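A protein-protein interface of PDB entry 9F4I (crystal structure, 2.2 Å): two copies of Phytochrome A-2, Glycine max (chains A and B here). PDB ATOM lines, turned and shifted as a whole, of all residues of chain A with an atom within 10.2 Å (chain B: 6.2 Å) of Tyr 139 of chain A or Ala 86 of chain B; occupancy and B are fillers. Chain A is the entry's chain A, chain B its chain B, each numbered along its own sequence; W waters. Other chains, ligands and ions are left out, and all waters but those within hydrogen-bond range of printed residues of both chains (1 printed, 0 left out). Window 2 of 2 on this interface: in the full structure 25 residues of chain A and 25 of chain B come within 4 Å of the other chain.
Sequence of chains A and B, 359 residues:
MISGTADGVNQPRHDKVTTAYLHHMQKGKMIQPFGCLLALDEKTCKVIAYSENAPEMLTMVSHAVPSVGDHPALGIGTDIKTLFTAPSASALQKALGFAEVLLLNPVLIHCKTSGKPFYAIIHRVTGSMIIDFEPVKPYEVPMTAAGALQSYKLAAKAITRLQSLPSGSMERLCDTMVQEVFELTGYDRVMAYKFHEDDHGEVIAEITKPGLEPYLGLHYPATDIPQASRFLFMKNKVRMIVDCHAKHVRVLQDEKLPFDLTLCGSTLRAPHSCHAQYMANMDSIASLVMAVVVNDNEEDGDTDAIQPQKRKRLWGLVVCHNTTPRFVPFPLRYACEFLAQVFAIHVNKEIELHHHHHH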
ATOM      1  N   LEU A 108      34.896   3.981 -13.181  1.00  0.00           N
ATOM      2  CA  LEU A 108      33.705   3.594 -12.449  1.00  0.00           C
ATOM      3  C   LEU A 108      33.202   2.275 -13.005  1.00  0.00           C
ATOM      4  O   LEU A 108      33.156   2.091 -14.220  1.00  0.00           O
ATOM      5  CB  LEU A 108      32.635   4.674 -12.570  1.00  0.00           C
ATOM      6  CG  LEU A 108      31.251   4.320 -12.023  1.00  0.00           C
ATOM      7  CD1 LEU A 108      31.321   3.822 -10.593  1.00  0.00           C
ATOM      8  CD2 LEU A 108      30.391   5.556 -12.121  1.00  0.00           C
ATOM      9  N   HIS A 110      30.444  -1.347 -12.240  1.00  0.00           N
ATOM     10  CA  HIS A 110      29.283  -1.895 -11.552  1.00  0.00           C
ATOM     11  C   HIS A 110      29.423  -3.408 -11.448  1.00  0.00           C
ATOM     12  O   HIS A 110      30.046  -4.046 -12.300  1.00  0.00           O
ATOM     13  CB  HIS A 110      27.952  -1.551 -12.279  1.00  0.00           C
ATOM     14  CG  HIS A 110      27.664  -0.085 -12.365  1.00  0.00           C
ATOM     15  ND1 HIS A 110      28.348   0.762 -13.213  1.00  0.00           N
ATOM     16  CD2 HIS A 110      26.760   0.686 -11.714  1.00  0.00           C
ATOM     17  CE1 HIS A 110      27.886   1.992 -13.069  1.00  0.00           C
ATOM     18  NE2 HIS A 110      26.917   1.972 -12.172  1.00  0.00           N
ATOM     19  N   GLY A 115      24.506  -4.154  -9.027  1.00  0.00           N
ATOM     20  CA  GLY A 115      24.682  -2.794  -9.477  1.00  0.00           C
ATOM     21  C   GLY A 115      25.355  -1.889  -8.470  1.00  0.00           C
ATOM     22  O   GLY A 115      25.207  -0.667  -8.563  1.00  0.00           O
ATOM     23  N   LYS A 116      26.058  -2.444  -7.493  1.00  0.00           N
ATOM     24  CA  LYS A 116      26.895  -1.612  -6.642  1.00  0.00           C
ATOM     25  C   LYS A 116      28.000  -0.979  -7.493  1.00  0.00           C
ATOM     26  O   LYS A 116      28.644  -1.674  -8.287  1.00  0.00           O
ATOM     27  CB  LYS A 116      27.496  -2.416  -5.484  1.00  0.00           C
ATOM     28  CG  LYS A 116      26.474  -2.841  -4.410  1.00  0.00           C
ATOM     29  CD  LYS A 116      27.103  -3.149  -3.052  1.00  0.00           C
ATOM     30  CE  LYS A 116      27.076  -4.646  -2.729  1.00  0.00           C
ATOM     31  NZ  LYS A 116      27.443  -4.999  -1.316  1.00  0.00           N
ATOM     32  N   PRO A 117      28.197   0.321  -7.414  1.00  0.00           N
ATOM     33  CA  PRO A 117      29.276   0.949  -8.190  1.00  0.00           C
ATOM     34  C   PRO A 117      30.550   1.157  -7.375  1.00  0.00           C
ATOM     35  O   PRO A 117      30.494   1.355  -6.159  1.00  0.00           O
ATOM     36  CB  PRO A 117      28.661   2.282  -8.621  1.00  0.00           C
ATOM     37  CG  PRO A 117      27.672   2.605  -7.546  1.00  0.00           C
ATOM     38  CD  PRO A 117      27.190   1.302  -6.959  1.00  0.00           C
ATOM     39  N   PRO A 135      34.645   2.445  -2.526  1.00  0.00           N
ATOM     40  CA  PRO A 135      33.178   2.456  -2.582  1.00  0.00           C
ATOM     41  C   PRO A 135      32.633   3.795  -3.036  1.00  0.00           C
ATOM     42  O   PRO A 135      33.164   4.856  -2.692  1.00  0.00           O
ATOM     43  CB  PRO A 135      32.764   2.148  -1.141  1.00  0.00           C
ATOM     44  CG  PRO A 135      33.873   2.786  -0.328  1.00  0.00           C
ATOM     45  CD  PRO A 135      35.145   2.702  -1.161  1.00  0.00           C
ATOM     46  N   VAL A 136      31.557   3.723  -3.824  1.00  0.00           N
ATOM     47  CA  VAL A 136      30.880   4.880  -4.396  1.00  0.00           C
ATOM     48  C   VAL A 136      29.381   4.750  -4.105  1.00  0.00           C
ATOM     49  O   VAL A 136      28.726   3.822  -4.598  1.00  0.00           O
ATOM     50  CB  VAL A 136      31.144   4.990  -5.912  1.00  0.00           C
ATOM     51  CG1 VAL A 136      30.100   5.838  -6.574  1.00  0.00           C
ATOM     52  CG2 VAL A 136      32.561   5.553  -6.167  1.00  0.00           C
ATOM     53  N   LYS A 137      28.851   5.674  -3.314  1.00  0.00           N
ATOM     54  CA  LYS A 137      27.432   5.691  -2.997  1.00  0.00           C
ATOM     55  C   LYS A 137      26.598   5.658  -4.289  1.00  0.00           C
ATOM     56  O   LYS A 137      26.931   6.352  -5.258  1.00  0.00           O
ATOM     57  CB  LYS A 137      27.095   6.937  -2.168  1.00  0.00           C
ATOM     58  CG  LYS A 137      27.937   7.101  -0.878  1.00  0.00           C
ATOM     59  CD  LYS A 137      27.422   8.258   0.006  1.00  0.00           C
ATOM     60  CE  LYS A 137      28.026   8.245   1.415  1.00  0.00           C
ATOM     61  NZ  LYS A 137      27.267   9.098   2.376  1.00  0.00           N
ATOM     62  N   PRO A 138      25.533   4.861  -4.349  1.00  0.00           N
ATOM     63  CA  PRO A 138      24.817   4.705  -5.629  1.00  0.00           C
ATOM     64  C   PRO A 138      24.057   5.946  -6.085  1.00  0.00           C
ATOM     65  O   PRO A 138      23.784   6.077  -7.287  1.00  0.00           O
ATOM     66  CB  PRO A 138      23.858   3.531  -5.364  1.00  0.00           C
ATOM     67  CG  PRO A 138      24.350   2.884  -4.087  1.00  0.00           C
ATOM     68  CD  PRO A 138      25.030   3.956  -3.299  1.00  0.00           C
ATOM     69  N   TYR A 139      23.705   6.863  -5.189  1.00  0.00           N
ATOM     70  CA  TYR A 139      22.915   8.021  -5.596  1.00  0.00           C
ATOM     71  C   TYR A 139      23.766   9.235  -5.921  1.00  0.00           C
ATOM     72  O   TYR A 139      23.210  10.277  -6.285  1.00  0.00           O
ATOM     73  CB  TYR A 139      21.885   8.377  -4.513  1.00  0.00           C
ATOM     74  CG  TYR A 139      20.543   7.741  -4.775  1.00  0.00           C
ATOM     75  CD1 TYR A 139      20.294   6.412  -4.418  1.00  0.00           C
ATOM     76  CD2 TYR A 139      19.523   8.459  -5.385  1.00  0.00           C
ATOM     77  CE1 TYR A 139      19.060   5.817  -4.665  1.00  0.00           C
ATOM     78  CE2 TYR A 139      18.282   7.875  -5.633  1.00  0.00           C
ATOM     79  CZ  TYR A 139      18.061   6.564  -5.274  1.00  0.00           C
ATOM     80  OH  TYR A 139      16.834   6.011  -5.540  1.00  0.00           O
ATOM     81  N   GLU A 140      25.093   9.114  -5.811  1.00  0.00           N
ATOM     82  CA  GLU A 140      26.030  10.150  -6.219  1.00  0.00           C
ATOM     83  C   GLU A 140      26.691   9.872  -7.568  1.00  0.00           C
ATOM     84  O   GLU A 140      27.406  10.741  -8.083  1.00  0.00           O
ATOM     85  CB  GLU A 140      27.106  10.340  -5.143  1.00  0.00           C
ATOM     86  CG  GLU A 140      26.564  10.774  -3.772  1.00  0.00           C
ATOM     87  CD  GLU A 140      26.826  12.231  -3.456  1.00  0.00           C
ATOM     88  OE1 GLU A 140      26.200  13.107  -4.084  1.00  0.00           O
ATOM     89  OE2 GLU A 140      27.671  12.498  -2.580  1.00  0.00           O
ATOM     90  N   VAL A 141      26.472   8.702  -8.157  1.00  0.00           N
ATOM     91  CA  VAL A 141      27.029   8.373  -9.470  1.00  0.00           C
ATOM     92  C   VAL A 141      26.670   9.428 -10.526  1.00  0.00           C
ATOM     93  O   VAL A 141      27.520   9.734 -11.371  1.00  0.00           O
ATOM     94  CB  VAL A 141      26.607   6.950  -9.890  1.00  0.00           C
ATOM     95  CG1 VAL A 141      26.898   6.701 -11.373  1.00  0.00           C
ATOM     96  CG2 VAL A 141      27.339   5.906  -9.038  1.00  0.00           C
ATOM     97  N   PRO A 142      25.474  10.033 -10.541  1.00  0.00           N
ATOM     98  CA  PRO A 142      25.265  11.170 -11.463  1.00  0.00           C
ATOM     99  C   PRO A 142      26.186  12.354 -11.196  1.00  0.00           C
ATOM    100  O   PRO A 142      26.460  13.141 -12.117  1.00  0.00           O
ATOM    101  CB  PRO A 142      23.793  11.560 -11.233  1.00  0.00           C
ATOM    102  CG  PRO A 142      23.156  10.371 -10.662  1.00  0.00           C
ATOM    103  CD  PRO A 142      24.214   9.647  -9.872  1.00  0.00           C
ATOM    104  N   MET A 143      26.666  12.507  -9.969  1.00  0.00           N
ATOM    105  CA  MET A 143      27.502  13.633  -9.582  1.00  0.00           C
ATOM    106  C   MET A 143      29.001  13.347  -9.673  1.00  0.00           C
ATOM    107  O   MET A 143      29.786  14.086  -9.075  1.00  0.00           O
ATOM    108  CB  MET A 143      27.162  14.046  -8.149  1.00  0.00           C
ATOM    109  CG  MET A 143      25.659  14.048  -7.825  1.00  0.00           C
ATOM    110  SD  MET A 143      24.664  14.892  -9.080  1.00  0.00           S
ATOM    111  CE  MET A 143      25.493  16.505  -9.197  1.00  0.00           C
ATOM    112  N   THR A 144      29.424  12.299 -10.391  1.00  0.00           N
ATOM    113  CA  THR A 144      30.839  11.915 -10.357  1.00  0.00           C
ATOM    114  C   THR A 144      31.722  12.961 -11.028  1.00  0.00           C
ATOM    115  O   THR A 144      32.677  13.469 -10.423  1.00  0.00           O
ATOM    116  CB  THR A 144      31.057  10.552 -11.018  1.00  0.00           C
ATOM    117  OG1 THR A 144      30.639  10.602 -12.394  1.00  0.00           O
ATOM    118  CG2 THR A 144      30.345   9.444 -10.252  1.00  0.00           C
ATOM    119  N   PHE B  84      13.694   9.680 -16.417  1.00  0.00           N
ATOM    120  CA  PHE B  84      15.057   9.252 -16.154  1.00  0.00           C
ATOM    121  C   PHE B  84      15.037   8.090 -15.177  1.00  0.00           C
ATOM    122  O   PHE B  84      13.972   7.693 -14.705  1.00  0.00           O
ATOM    123  CB  PHE B  84      15.896  10.422 -15.618  1.00  0.00           C
ATOM    124  CG  PHE B  84      15.770  11.667 -16.446  1.00  0.00           C
ATOM    125  CD1 PHE B  84      16.288  11.713 -17.740  1.00  0.00           C
ATOM    126  CD2 PHE B  84      15.097  12.783 -15.949  1.00  0.00           C
ATOM    127  CE1 PHE B  84      16.139  12.858 -18.533  1.00  0.00           C
ATOM    128  CE2 PHE B  84      14.951  13.953 -16.724  1.00  0.00           C
ATOM    129  CZ  PHE B  84      15.471  13.992 -18.019  1.00  0.00           C
ATOM    130  N   THR B  85      16.215   7.516 -14.885  1.00  0.00           N
ATOM    131  CA  THR B  85      16.245   6.573 -13.774  1.00  0.00           C
ATOM    132  C   THR B  85      16.081   7.326 -12.458  1.00  0.00           C
ATOM    133  O   THR B  85      16.215   8.549 -12.396  1.00  0.00           O
ATOM    134  CB  THR B  85      17.525   5.707 -13.758  1.00  0.00           C
ATOM    135  OG1 THR B  85      18.710   6.509 -13.672  1.00  0.00           O
ATOM    136  CG2 THR B  85      17.601   4.798 -14.988  1.00  0.00           C
ATOM    137  N   ALA B  86      15.759   6.589 -11.390  1.00  0.00           N
ATOM    138  CA  ALA B  86      15.543   7.248 -10.100  1.00  0.00           C
ATOM    139  C   ALA B  86      16.715   8.117  -9.668  1.00  0.00           C
ATOM    140  O   ALA B  86      16.496   9.310  -9.422  1.00  0.00           O
ATOM    141  CB  ALA B  86      15.215   6.202  -9.023  1.00  0.00           C
ATOM    142  N   PRO B  87      17.960   7.619  -9.590  1.00  0.00           N
ATOM    143  CA  PRO B  87      19.046   8.438  -9.006  1.00  0.00           C
ATOM    144  C   PRO B  87      19.515   9.615  -9.878  1.00  0.00           C
ATOM    145  O   PRO B  87      20.088  10.565  -9.334  1.00  0.00           O
ATOM    146  CB  PRO B  87      20.166   7.413  -8.804  1.00  0.00           C
ATOM    147  CG  PRO B  87      19.949   6.458  -9.996  1.00  0.00           C
ATOM    148  CD  PRO B  87      18.455   6.281  -9.979  1.00  0.00           C
ATOM    149  N   SER B  88      19.362   9.552 -11.202  1.00  0.00           N
ATOM    150  CA  SER B  88      19.462  10.762 -12.014  1.00  0.00           C
ATOM    151  C   SER B  88      18.344  11.735 -11.651  1.00  0.00           C
ATOM    152  O   SER B  88      18.594  12.901 -11.324  1.00  0.00           O
ATOM    153  CB  SER B  88      19.404  10.400 -13.510  1.00  0.00           C
ATOM    154  OG  SER B  88      19.276   8.986 -13.706  1.00  0.00           O
ATOM    155  N   ALA B  89      17.095  11.259 -11.681  1.00  0.00           N
ATOM    156  CA  ALA B  89      15.964  12.072 -11.237  1.00  0.00           C
ATOM    157  C   ALA B  89      16.185  12.613  -9.833  1.00  0.00           C
ATOM    158  O   ALA B  89      16.004  13.806  -9.578  1.00  0.00           O
ATOM    159  CB  ALA B  89      14.675  11.254 -11.296  1.00  0.00           C
ATOM    160  N   SER B  90      16.578  11.747  -8.904  1.00  0.00           N
ATOM    161  CA  SER B  90      16.860  12.217  -7.549  1.00  0.00           C
ATOM    162  C   SER B  90      17.998  13.232  -7.513  1.00  0.00           C
ATOM    163  O   SER B  90      18.014  14.104  -6.645  1.00  0.00           O
ATOM    164  CB  SER B  90      17.198  11.028  -6.659  1.00  0.00           C
ATOM    165  OG  SER B  90      17.675  11.470  -5.407  1.00  0.00           O
ATOM    166  N   ALA B  91      18.955  13.122  -8.442  1.00  0.00           N
ATOM    167  CA  ALA B  91      20.143  13.973  -8.495  1.00  0.00           C
ATOM    168  C   ALA B  91      19.856  15.346  -9.063  1.00  0.00           C
ATOM    169  O   ALA B  91      20.546  16.305  -8.702  1.00  0.00           O
ATOM    170  CB  ALA B  91      21.227  13.302  -9.341  1.00  0.00           C
ATOM    171  N   LYS B 112      15.015   6.623 -18.526  1.00  0.00           N
ATOM    172  CA  LYS B 112      14.347   5.494 -17.877  1.00  0.00           C
ATOM    173  C   LYS B 112      14.413   4.215 -18.712  1.00  0.00           C
ATOM    174  O   LYS B 112      14.993   3.203 -18.297  1.00  0.00           O
ATOM    175  CB  LYS B 112      12.887   5.860 -17.605  1.00  0.00           C
ATOM    176  CG  LYS B 112      12.347   5.236 -16.361  1.00  0.00           C
ATOM    177  CD  LYS B 112      11.320   6.115 -15.696  1.00  0.00           C
ATOM    178  CE  LYS B 112      11.059   5.713 -14.254  1.00  0.00           C
ATOM    179  NZ  LYS B 112       9.925   4.765 -14.218  1.00  0.00           N
HETATM  180  O   HOH W   1      20.972  11.296  -6.490  1.00  0.00           O
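Tyr 139 of chain A touches three residues of chain B. Ala 86 of chain B touches one residue of chain A. No residue of chain A comes within 4 Å of Thr 85 of chain B. Of chain A, only Tyr 139 and Pro 142 come within 4 Å of Pro 87 of chain B. Ser 88 of chain B touches just one residue of chain A: Pro 142 (3.9 Å). No residue of chain A comes within 4 Å of Ala 89 of chain B. Printed residues of chain A within 4 Å of Ser 90 of chain B: Tyr 139. Of the printed residues of chain B, Pro 142 of chain A touches Pro 87, Ser 88 and Ala 91. Of the printed residues of chain B, Met 143 of chain A touches Ala 91. Of the printed residues of chain A, Ala 91 of chain B touches Pro 142 (3.6 Å) and Met 143 (3.8 Å). Val 141 of chain A touches none of the printed residues of chain B. Glu 140 of chain A touches none of the printed residues of chain B. The nearest residue of chain A that does not touch Ala 86 of chain B is Pro 142 of chain A (6.9 Å).
No position is printed for both chains.
Along chain B the printed residues that touch a printed residue of chain A span positions 86 to 91. Hydrophobic or aromatic side chains of chain A that line the printed part of chain B: Tyr 139, Pro 142 and Met 143.
The side-chain hydroxyl (OG1) of Thr 85 of chain B lies within hydrogen-bond range of the side-chain hydroxyl (OG) of Ser 88 of chain B (2.5 Å).
Among the printed residues, pairs that only touch across the chains: Tyr 139 of chain A with Ala 86 of chain B, Tyr 139 of chain A with Pro 87 of chain B, Tyr 139 of chain A with Ser 90 of chain B, Pro 142 of chain A with Pro 87 of chain B, Pro 142 of chain A with Ser 88 of chain B, Pro 142 of chain A with Ala 91 of chain B and Met 143 of chain A with Ala 91 of chain B.
Water W1 lies within hydrogen-bond range of O of Tyr 139 of chain A (2.5 Å), O of Pro 87 of chain B (3.1 Å), N of Ala 91 of chain B (3.3 Å) and OG of Ser 90 of chain B (3.5 Å).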
